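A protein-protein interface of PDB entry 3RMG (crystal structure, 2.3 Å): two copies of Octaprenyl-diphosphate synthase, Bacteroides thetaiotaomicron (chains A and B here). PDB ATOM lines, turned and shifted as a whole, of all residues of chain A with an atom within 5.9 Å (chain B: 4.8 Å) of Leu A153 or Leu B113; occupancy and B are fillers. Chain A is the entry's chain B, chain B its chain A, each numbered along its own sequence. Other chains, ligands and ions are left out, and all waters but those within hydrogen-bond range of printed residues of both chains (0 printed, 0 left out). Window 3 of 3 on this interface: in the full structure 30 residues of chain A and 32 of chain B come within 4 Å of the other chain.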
ATOM      1  N   HIS A  86       5.417  -3.686  -2.080  1.00  0.00           N
ATOM      2  CA  HIS A  86       6.455  -4.321  -2.891  1.00  0.00           C
ATOM      3  C   HIS A  86       5.865  -5.022  -4.121  1.00  0.00           C
ATOM      4  O   HIS A  86       6.509  -5.117  -5.157  1.00  0.00           O
ATOM      5  CB  HIS A  86       7.315  -5.293  -2.066  1.00  0.00           C
ATOM      6  CG  HIS A  86       8.405  -4.623  -1.282  1.00  0.00           C
ATOM      7  ND1 HIS A  86       9.078  -5.245  -0.254  1.00  0.00           N
ATOM      8  CD2 HIS A  86       8.939  -3.382  -1.379  1.00  0.00           C
ATOM      9  CE1 HIS A  86       9.980  -4.420   0.247  1.00  0.00           C
ATOM     10  NE2 HIS A  86       9.913  -3.280  -0.417  1.00  0.00           N
ATOM     11  N   ASP A  87       4.635  -5.508  -4.021  1.00  0.00           N
ATOM     12  CA  ASP A  87       4.022  -6.167  -5.162  1.00  0.00           C
ATOM     13  C   ASP A  87       3.771  -5.197  -6.329  1.00  0.00           C
ATOM     14  O   ASP A  87       3.445  -5.619  -7.438  1.00  0.00           O
ATOM     15  CB  ASP A  87       2.736  -6.893  -4.747  1.00  0.00           C
ATOM     16  CG  ASP A  87       3.011  -8.157  -3.926  1.00  0.00           C
ATOM     17  OD1 ASP A  87       4.152  -8.324  -3.428  1.00  0.00           O
ATOM     18  OD2 ASP A  87       2.081  -8.985  -3.776  1.00  0.00           O
ATOM     19  N   VAL A  90       5.674  -4.961  -9.808  1.00  0.00           N
ATOM     20  CA  VAL A  90       5.191  -5.859 -10.863  1.00  0.00           C
ATOM     21  C   VAL A  90       4.784  -5.082 -12.113  1.00  0.00           C
ATOM     22  O   VAL A  90       4.643  -3.857 -12.080  1.00  0.00           O
ATOM     23  CB  VAL A  90       3.988  -6.717 -10.380  1.00  0.00           C
ATOM     24  CG1 VAL A  90       2.713  -5.874 -10.308  1.00  0.00           C
ATOM     25  CG2 VAL A  90       3.781  -7.923 -11.290  1.00  0.00           C
ATOM     26  N   ALA A 146       7.123 -14.125   1.250  1.00  0.00           N
ATOM     27  CA  ALA A 146       8.107 -13.872   0.213  1.00  0.00           C
ATOM     28  C   ALA A 146       8.202 -15.090  -0.692  1.00  0.00           C
ATOM     29  O   ALA A 146       7.727 -15.068  -1.830  1.00  0.00           O
ATOM     30  CB  ALA A 146       9.453 -13.551   0.826  1.00  0.00           C
ATOM     31  N   GLU A 147       8.811 -16.151  -0.171  1.00  0.00           N
ATOM     32  CA  GLU A 147       8.886 -17.434  -0.858  1.00  0.00           C
ATOM     33  C   GLU A 147       7.591 -17.779  -1.604  1.00  0.00           C
ATOM     34  O   GLU A 147       7.619 -18.421  -2.653  1.00  0.00           O
ATOM     35  CB  GLU A 147       9.215 -18.534   0.149  1.00  0.00           C
ATOM     36  CG  GLU A 147       9.461 -19.886  -0.475  1.00  0.00           C
ATOM     37  CD  GLU A 147       8.816 -21.009   0.316  1.00  0.00           C
ATOM     38  OE1 GLU A 147       9.484 -22.043   0.527  1.00  0.00           O
ATOM     39  OE2 GLU A 147       7.641 -20.855   0.726  1.00  0.00           O
ATOM     40  N   GLY A 148       6.457 -17.351  -1.060  1.00  0.00           N
ATOM     41  CA  GLY A 148       5.158 -17.602  -1.685  1.00  0.00           C
ATOM     42  C   GLY A 148       4.865 -16.717  -2.890  1.00  0.00           C
ATOM     43  O   GLY A 148       3.855 -16.897  -3.577  1.00  0.00           O
ATOM     44  N   GLU A 149       5.744 -15.753  -3.146  1.00  0.00           N
ATOM     45  CA  GLU A 149       5.624 -14.919  -4.336  1.00  0.00           C
ATOM     46  C   GLU A 149       6.520 -15.453  -5.449  1.00  0.00           C
ATOM     47  O   GLU A 149       6.227 -15.266  -6.630  1.00  0.00           O
ATOM     48  CB  GLU A 149       5.951 -13.452  -4.031  1.00  0.00           C
ATOM     49  CG  GLU A 149       4.786 -12.650  -3.455  1.00  0.00           C
ATOM     50  CD  GLU A 149       3.665 -12.407  -4.463  1.00  0.00           C
ATOM     51  OE1 GLU A 149       3.256 -11.237  -4.626  1.00  0.00           O
ATOM     52  OE2 GLU A 149       3.189 -13.378  -5.091  1.00  0.00           O
ATOM     53  N   LEU A 150       7.609 -16.117  -5.069  1.00  0.00           N
ATOM     54  CA  LEU A 150       8.450 -16.816  -6.039  1.00  0.00           C
ATOM     55  C   LEU A 150       7.808 -18.150  -6.415  1.00  0.00           C
ATOM     56  O   LEU A 150       8.177 -18.770  -7.412  1.00  0.00           O
ATOM     57  CB  LEU A 150       9.859 -17.033  -5.486  1.00  0.00           C
ATOM     58  CG  LEU A 150      10.646 -15.730  -5.382  1.00  0.00           C
ATOM     59  CD1 LEU A 150       9.705 -14.660  -4.905  1.00  0.00           C
ATOM     60  CD2 LEU A 150      11.860 -15.850  -4.461  1.00  0.00           C
ATOM     61  N   LEU A 151       6.846 -18.578  -5.599  1.00  0.00           N
ATOM     62  CA  LEU A 151       6.084 -19.801  -5.848  1.00  0.00           C
ATOM     63  C   LEU A 151       5.031 -19.560  -6.917  1.00  0.00           C
ATOM     64  O   LEU A 151       4.622 -20.483  -7.621  1.00  0.00           O
ATOM     65  CB  LEU A 151       5.396 -20.285  -4.568  1.00  0.00           C
ATOM     66  CG  LEU A 151       4.305 -21.341  -4.767  1.00  0.00           C
ATOM     67  CD1 LEU A 151       4.899 -22.640  -5.297  1.00  0.00           C
ATOM     68  CD2 LEU A 151       3.526 -21.583  -3.478  1.00  0.00           C
ATOM     69  N   GLN A 152       4.582 -18.314  -7.019  1.00  0.00           N
ATOM     70  CA  GLN A 152       3.628 -17.930  -8.045  1.00  0.00           C
ATOM     71  C   GLN A 152       4.367 -17.439  -9.286  1.00  0.00           C
ATOM     72  O   GLN A 152       3.908 -17.637 -10.410  1.00  0.00           O
ATOM     73  CB  GLN A 152       2.691 -16.845  -7.520  1.00  0.00           C
ATOM     74  CG  GLN A 152       1.423 -16.682  -8.331  1.00  0.00           C
ATOM     75  CD  GLN A 152       0.388 -15.843  -7.617  1.00  0.00           C
ATOM     76  OE1 GLN A 152      -0.814 -16.026  -7.808  1.00  0.00           O
ATOM     77  NE2 GLN A 152       0.848 -14.918  -6.778  1.00  0.00           N
ATOM     78  N   LEU A 153       5.521 -16.810  -9.074  1.00  0.00           N
ATOM     79  CA  LEU A 153       6.342 -16.308 -10.173  1.00  0.00           C
ATOM     80  C   LEU A 153       7.213 -17.396 -10.812  1.00  0.00           C
ATOM     81  O   LEU A 153       7.966 -17.129 -11.751  1.00  0.00           O
ATOM     82  CB  LEU A 153       7.212 -15.139  -9.704  1.00  0.00           C
ATOM     83  CG  LEU A 153       6.486 -13.822  -9.414  1.00  0.00           C
ATOM     84  CD1 LEU A 153       7.365 -12.899  -8.592  1.00  0.00           C
ATOM     85  CD2 LEU A 153       6.048 -13.138 -10.703  1.00  0.00           C
ATOM     86  N   SER A 154       7.020 -18.610 -10.325  1.00  0.00           N
ATOM     87  CA  SER A 154       7.641 -19.782 -10.879  1.00  0.00           C
ATOM     88  C   SER A 154       6.525 -20.599 -11.504  1.00  0.00           C
ATOM     89  O   SER A 154       6.772 -21.494 -12.281  1.00  0.00           O
ATOM     90  CB  SER A 154       8.354 -20.582  -9.812  1.00  0.00           C
ATOM     91  OG  SER A 154       9.744 -20.340  -9.884  1.00  0.00           O
ATOM     92  N   ASN A 155       5.303 -20.261 -11.098  1.00  0.00           N
ATOM     93  CA  ASN A 155       4.056 -20.872 -11.554  1.00  0.00           C
ATOM     94  C   ASN A 155       3.775 -20.634 -13.033  1.00  0.00           C
ATOM     95  O   ASN A 155       3.230 -21.495 -13.724  1.00  0.00           O
ATOM     96  CB  ASN A 155       2.880 -20.379 -10.711  1.00  0.00           C
ATOM     97  CG  ASN A 155       1.558 -20.980 -11.146  1.00  0.00           C
ATOM     98  OD1 ASN A 155       1.502 -21.767 -12.091  1.00  0.00           O
ATOM     99  ND2 ASN A 155       0.484 -20.611 -10.457  1.00  0.00           N
ATOM    100  N   VAL A 156       4.145 -19.448 -13.505  1.00  0.00           N
ATOM    101  CA  VAL A 156       3.918 -19.047 -14.885  1.00  0.00           C
ATOM    102  C   VAL A 156       4.604 -20.020 -15.831  1.00  0.00           C
ATOM    103  O   VAL A 156       4.085 -20.322 -16.905  1.00  0.00           O
ATOM    104  CB  VAL A 156       4.441 -17.625 -15.155  1.00  0.00           C
ATOM    105  CG1 VAL A 156       4.255 -17.260 -16.620  1.00  0.00           C
ATOM    106  CG2 VAL A 156       3.739 -16.622 -14.254  1.00  0.00           C
ATOM    107  N   SER A 157       5.769 -20.512 -15.430  1.00  0.00           N
ATOM    108  CA  SER A 157       6.499 -21.457 -16.257  1.00  0.00           C
ATOM    109  C   SER A 157       5.626 -22.691 -16.463  1.00  0.00           C
ATOM    110  O   SER A 157       5.589 -23.253 -17.558  1.00  0.00           O
ATOM    111  CB  SER A 157       7.821 -21.846 -15.596  1.00  0.00           C
ATOM    112  OG  SER A 157       7.601 -22.448 -14.332  1.00  0.00           O
ATOM    113  N   LYS B 109      11.899  -7.557 -10.404  1.00  0.00           N
ATOM    114  CA  LYS B 109      10.838  -8.022  -9.472  1.00  0.00           C
ATOM    115  C   LYS B 109      11.123  -9.077  -8.376  1.00  0.00           C
ATOM    116  O   LYS B 109      10.778  -8.900  -7.229  1.00  0.00           O
ATOM    117  CB  LYS B 109       9.602  -8.466 -10.249  1.00  0.00           C
ATOM    118  N   VAL B 110      11.777 -10.154  -8.743  1.00  0.00           N
ATOM    119  CA  VAL B 110      12.242 -11.239  -7.879  1.00  0.00           C
ATOM    120  C   VAL B 110      13.342 -10.791  -6.912  1.00  0.00           C
ATOM    121  O   VAL B 110      13.372 -11.220  -5.756  1.00  0.00           O
ATOM    122  CB  VAL B 110      12.733 -12.459  -8.702  1.00  0.00           C
ATOM    123  CG1 VAL B 110      13.420 -13.465  -7.800  1.00  0.00           C
ATOM    124  CG2 VAL B 110      11.571 -13.113  -9.446  1.00  0.00           C
ATOM    125  N   SER B 111      14.234  -9.924  -7.385  1.00  0.00           N
ATOM    126  CA  SER B 111      15.336  -9.453  -6.561  1.00  0.00           C
ATOM    127  C   SER B 111      14.834  -8.650  -5.355  1.00  0.00           C
ATOM    128  O   SER B 111      15.451  -8.676  -4.286  1.00  0.00           O
ATOM    129  CB  SER B 111      16.338  -8.641  -7.387  1.00  0.00           C
ATOM    130  OG  SER B 111      15.987  -7.268  -7.436  1.00  0.00           O
ATOM    131  N   VAL B 112      13.719  -7.940  -5.522  1.00  0.00           N
ATOM    132  CA  VAL B 112      13.081  -7.263  -4.395  1.00  0.00           C
ATOM    133  C   VAL B 112      12.523  -8.311  -3.456  1.00  0.00           C
ATOM    134  O   VAL B 112      12.590  -8.173  -2.233  1.00  0.00           O
ATOM    135  CB  VAL B 112      11.936  -6.321  -4.845  1.00  0.00           C
ATOM    136  CG1 VAL B 112      10.915  -6.151  -3.734  1.00  0.00           C
ATOM    137  CG2 VAL B 112      12.489  -4.964  -5.251  1.00  0.00           C
ATOM    138  N   LEU B 113      11.971  -9.371  -4.031  1.00  0.00           N
ATOM    139  CA  LEU B 113      11.404 -10.440  -3.217  1.00  0.00           C
ATOM    140  C   LEU B 113      12.509 -11.260  -2.553  1.00  0.00           C
ATOM    141  O   LEU B 113      12.364 -11.710  -1.412  1.00  0.00           O
ATOM    142  CB  LEU B 113      10.477 -11.334  -4.046  1.00  0.00           C
ATOM    143  CG  LEU B 113       9.128 -10.715  -4.437  1.00  0.00           C
ATOM    144  CD1 LEU B 113       8.327 -11.675  -5.323  1.00  0.00           C
ATOM    145  CD2 LEU B 113       8.320 -10.311  -3.192  1.00  0.00           C
ATOM    146  N   ALA B 114      13.611 -11.444  -3.272  1.00  0.00           N
ATOM    147  CA  ALA B 114      14.779 -12.102  -2.708  1.00  0.00           C
ATOM    148  C   ALA B 114      15.252 -11.302  -1.493  1.00  0.00           C
ATOM    149  O   ALA B 114      15.357 -11.833  -0.386  1.00  0.00           O
ATOM    150  CB  ALA B 114      15.884 -12.215  -3.751  1.00  0.00           C
ATOM    151  N   GLY B 115      15.515 -10.018  -1.712  1.00  0.00           N
ATOM    152  CA  GLY B 115      15.832  -9.105  -0.624  1.00  0.00           C
ATOM    153  C   GLY B 115      14.861  -9.210   0.535  1.00  0.00           C
ATOM    154  O   GLY B 115      15.275  -9.207   1.693  1.00  0.00           O
ATOM    155  N   ASP B 116      13.564  -9.303   0.241  1.00  0.00           N
ATOM    156  CA  ASP B 116      12.564  -9.389   1.310  1.00  0.00           C
ATOM    157  C   ASP B 116      12.704 -10.714   2.071  1.00  0.00           C
ATOM    158  O   ASP B 116      12.497 -10.771   3.288  1.00  0.00           O
ATOM    159  CB  ASP B 116      11.138  -9.228   0.763  1.00  0.00           C
ATOM    160  CG  ASP B 116      10.825  -7.797   0.324  1.00  0.00           C
ATOM    161  OD1 ASP B 116      11.688  -6.911   0.513  1.00  0.00           O
ATOM    162  OD2 ASP B 116       9.710  -7.562  -0.212  1.00  0.00           O
ATOM    163  N   TYR B 117      13.049 -11.775   1.345  1.00  0.00           N
ATOM    164  CA  TYR B 117      13.313 -13.073   1.958  1.00  0.00           C
ATOM    165  C   TYR B 117      14.522 -12.990   2.882  1.00  0.00           C
ATOM    166  O   TYR B 117      14.399 -13.184   4.095  1.00  0.00           O
ATOM    167  CB  TYR B 117      13.558 -14.143   0.894  1.00  0.00           C
ATOM    168  CG  TYR B 117      13.640 -15.537   1.468  1.00  0.00           C
ATOM    169  CD1 TYR B 117      12.546 -16.101   2.108  1.00  0.00           C
ATOM    170  CD2 TYR B 117      14.803 -16.289   1.369  1.00  0.00           C
ATOM    171  CE1 TYR B 117      12.602 -17.372   2.639  1.00  0.00           C
ATOM    172  CE2 TYR B 117      14.872 -17.568   1.895  1.00  0.00           C
ATOM    173  CZ  TYR B 117      13.765 -18.102   2.532  1.00  0.00           C
ATOM    174  OH  TYR B 117      13.812 -19.374   3.064  1.00  0.00           O
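The side-chain carboxylate (OD2) of Asp B116 lies within hydrogen-bond range of a ring nitrogen (ND1) of His A86 (2.4 Å).
The side-chain carboxylate (OD2) of Asp A87 sits close to the side-chain carboxylate (OE1) of Glu A149, 2.7 Å away. The side-chain amide nitrogen of Gln A152 sits at hydrogen-bond distance from the side-chain carboxylate of Glu A149 (3.3 Å). The backbone carbonyl oxygen (O) of Leu A150 sits close to the side-chain hydroxyl (OG) of Ser A154, 3.3 Å away.
Among the printed residues, pairs that only touch across the chains: His A86 with Val B112 (3.8 Å), Glu A149 with Leu B113 (3.2 Å), Leu A150 with Leu B113 (3.3 Å) and Leu A153 with Leu B113 (3.6 Å).
Leu A153 touches just one residue of chain B: Leu B113. Of the printed residues of chain A, Leu B113 touches Glu A149 (3.2 Å), Leu A150 (3.3 Å) and Leu A153 (3.6 Å). Printed residues of chain A within 4 Å of Val B112: His A86 (3.8 Å). Printed residues of chain B within 4 Å of Leu A150: Leu B113 (3.3 Å). Printed residues of chain B within 4 Å of Glu A149: Leu B113. Of the printed residues of chain B, His A86 touches Val B112 and Asp B116. Of the printed residues of chain A, Asp B116 touches His A86. Gly A148 touches none of the printed residues of chain B. Val A156 touches none of the printed residues of chain B. The nearest residue of chain B that does not touch Leu A153 is Val B110 (4.3 Å). The nearest residue of chain A that does not touch Leu B113 is Ala A146 (4.1 Å). The nearest printed residue of chain A that does not touch Val B112 is Asp A87 (6.3 Å).
Of the 9 printed residues of chain B, 3 touch a printed residue of chain A. Hydrophobic or aromatic side chains of chain B that line the printed part of chain A: Val B112 and Leu B113. Printed residues of chain A that touch a printed residue of chain B: His A86, Glu A149, Leu A150 and Leu A153. Hydrophobic or aromatic side chains of chain A within 4 Å of the printed part of chain B: His A86, Leu A150 and Leu A153. Among the printed residues, 5 pairs touch across the chains. Among the printed residues, no Asp or Glu carboxylate lies within 4 Å of a Lys or Arg side-chain nitrogen of the other chain.
No position is printed for both chains.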
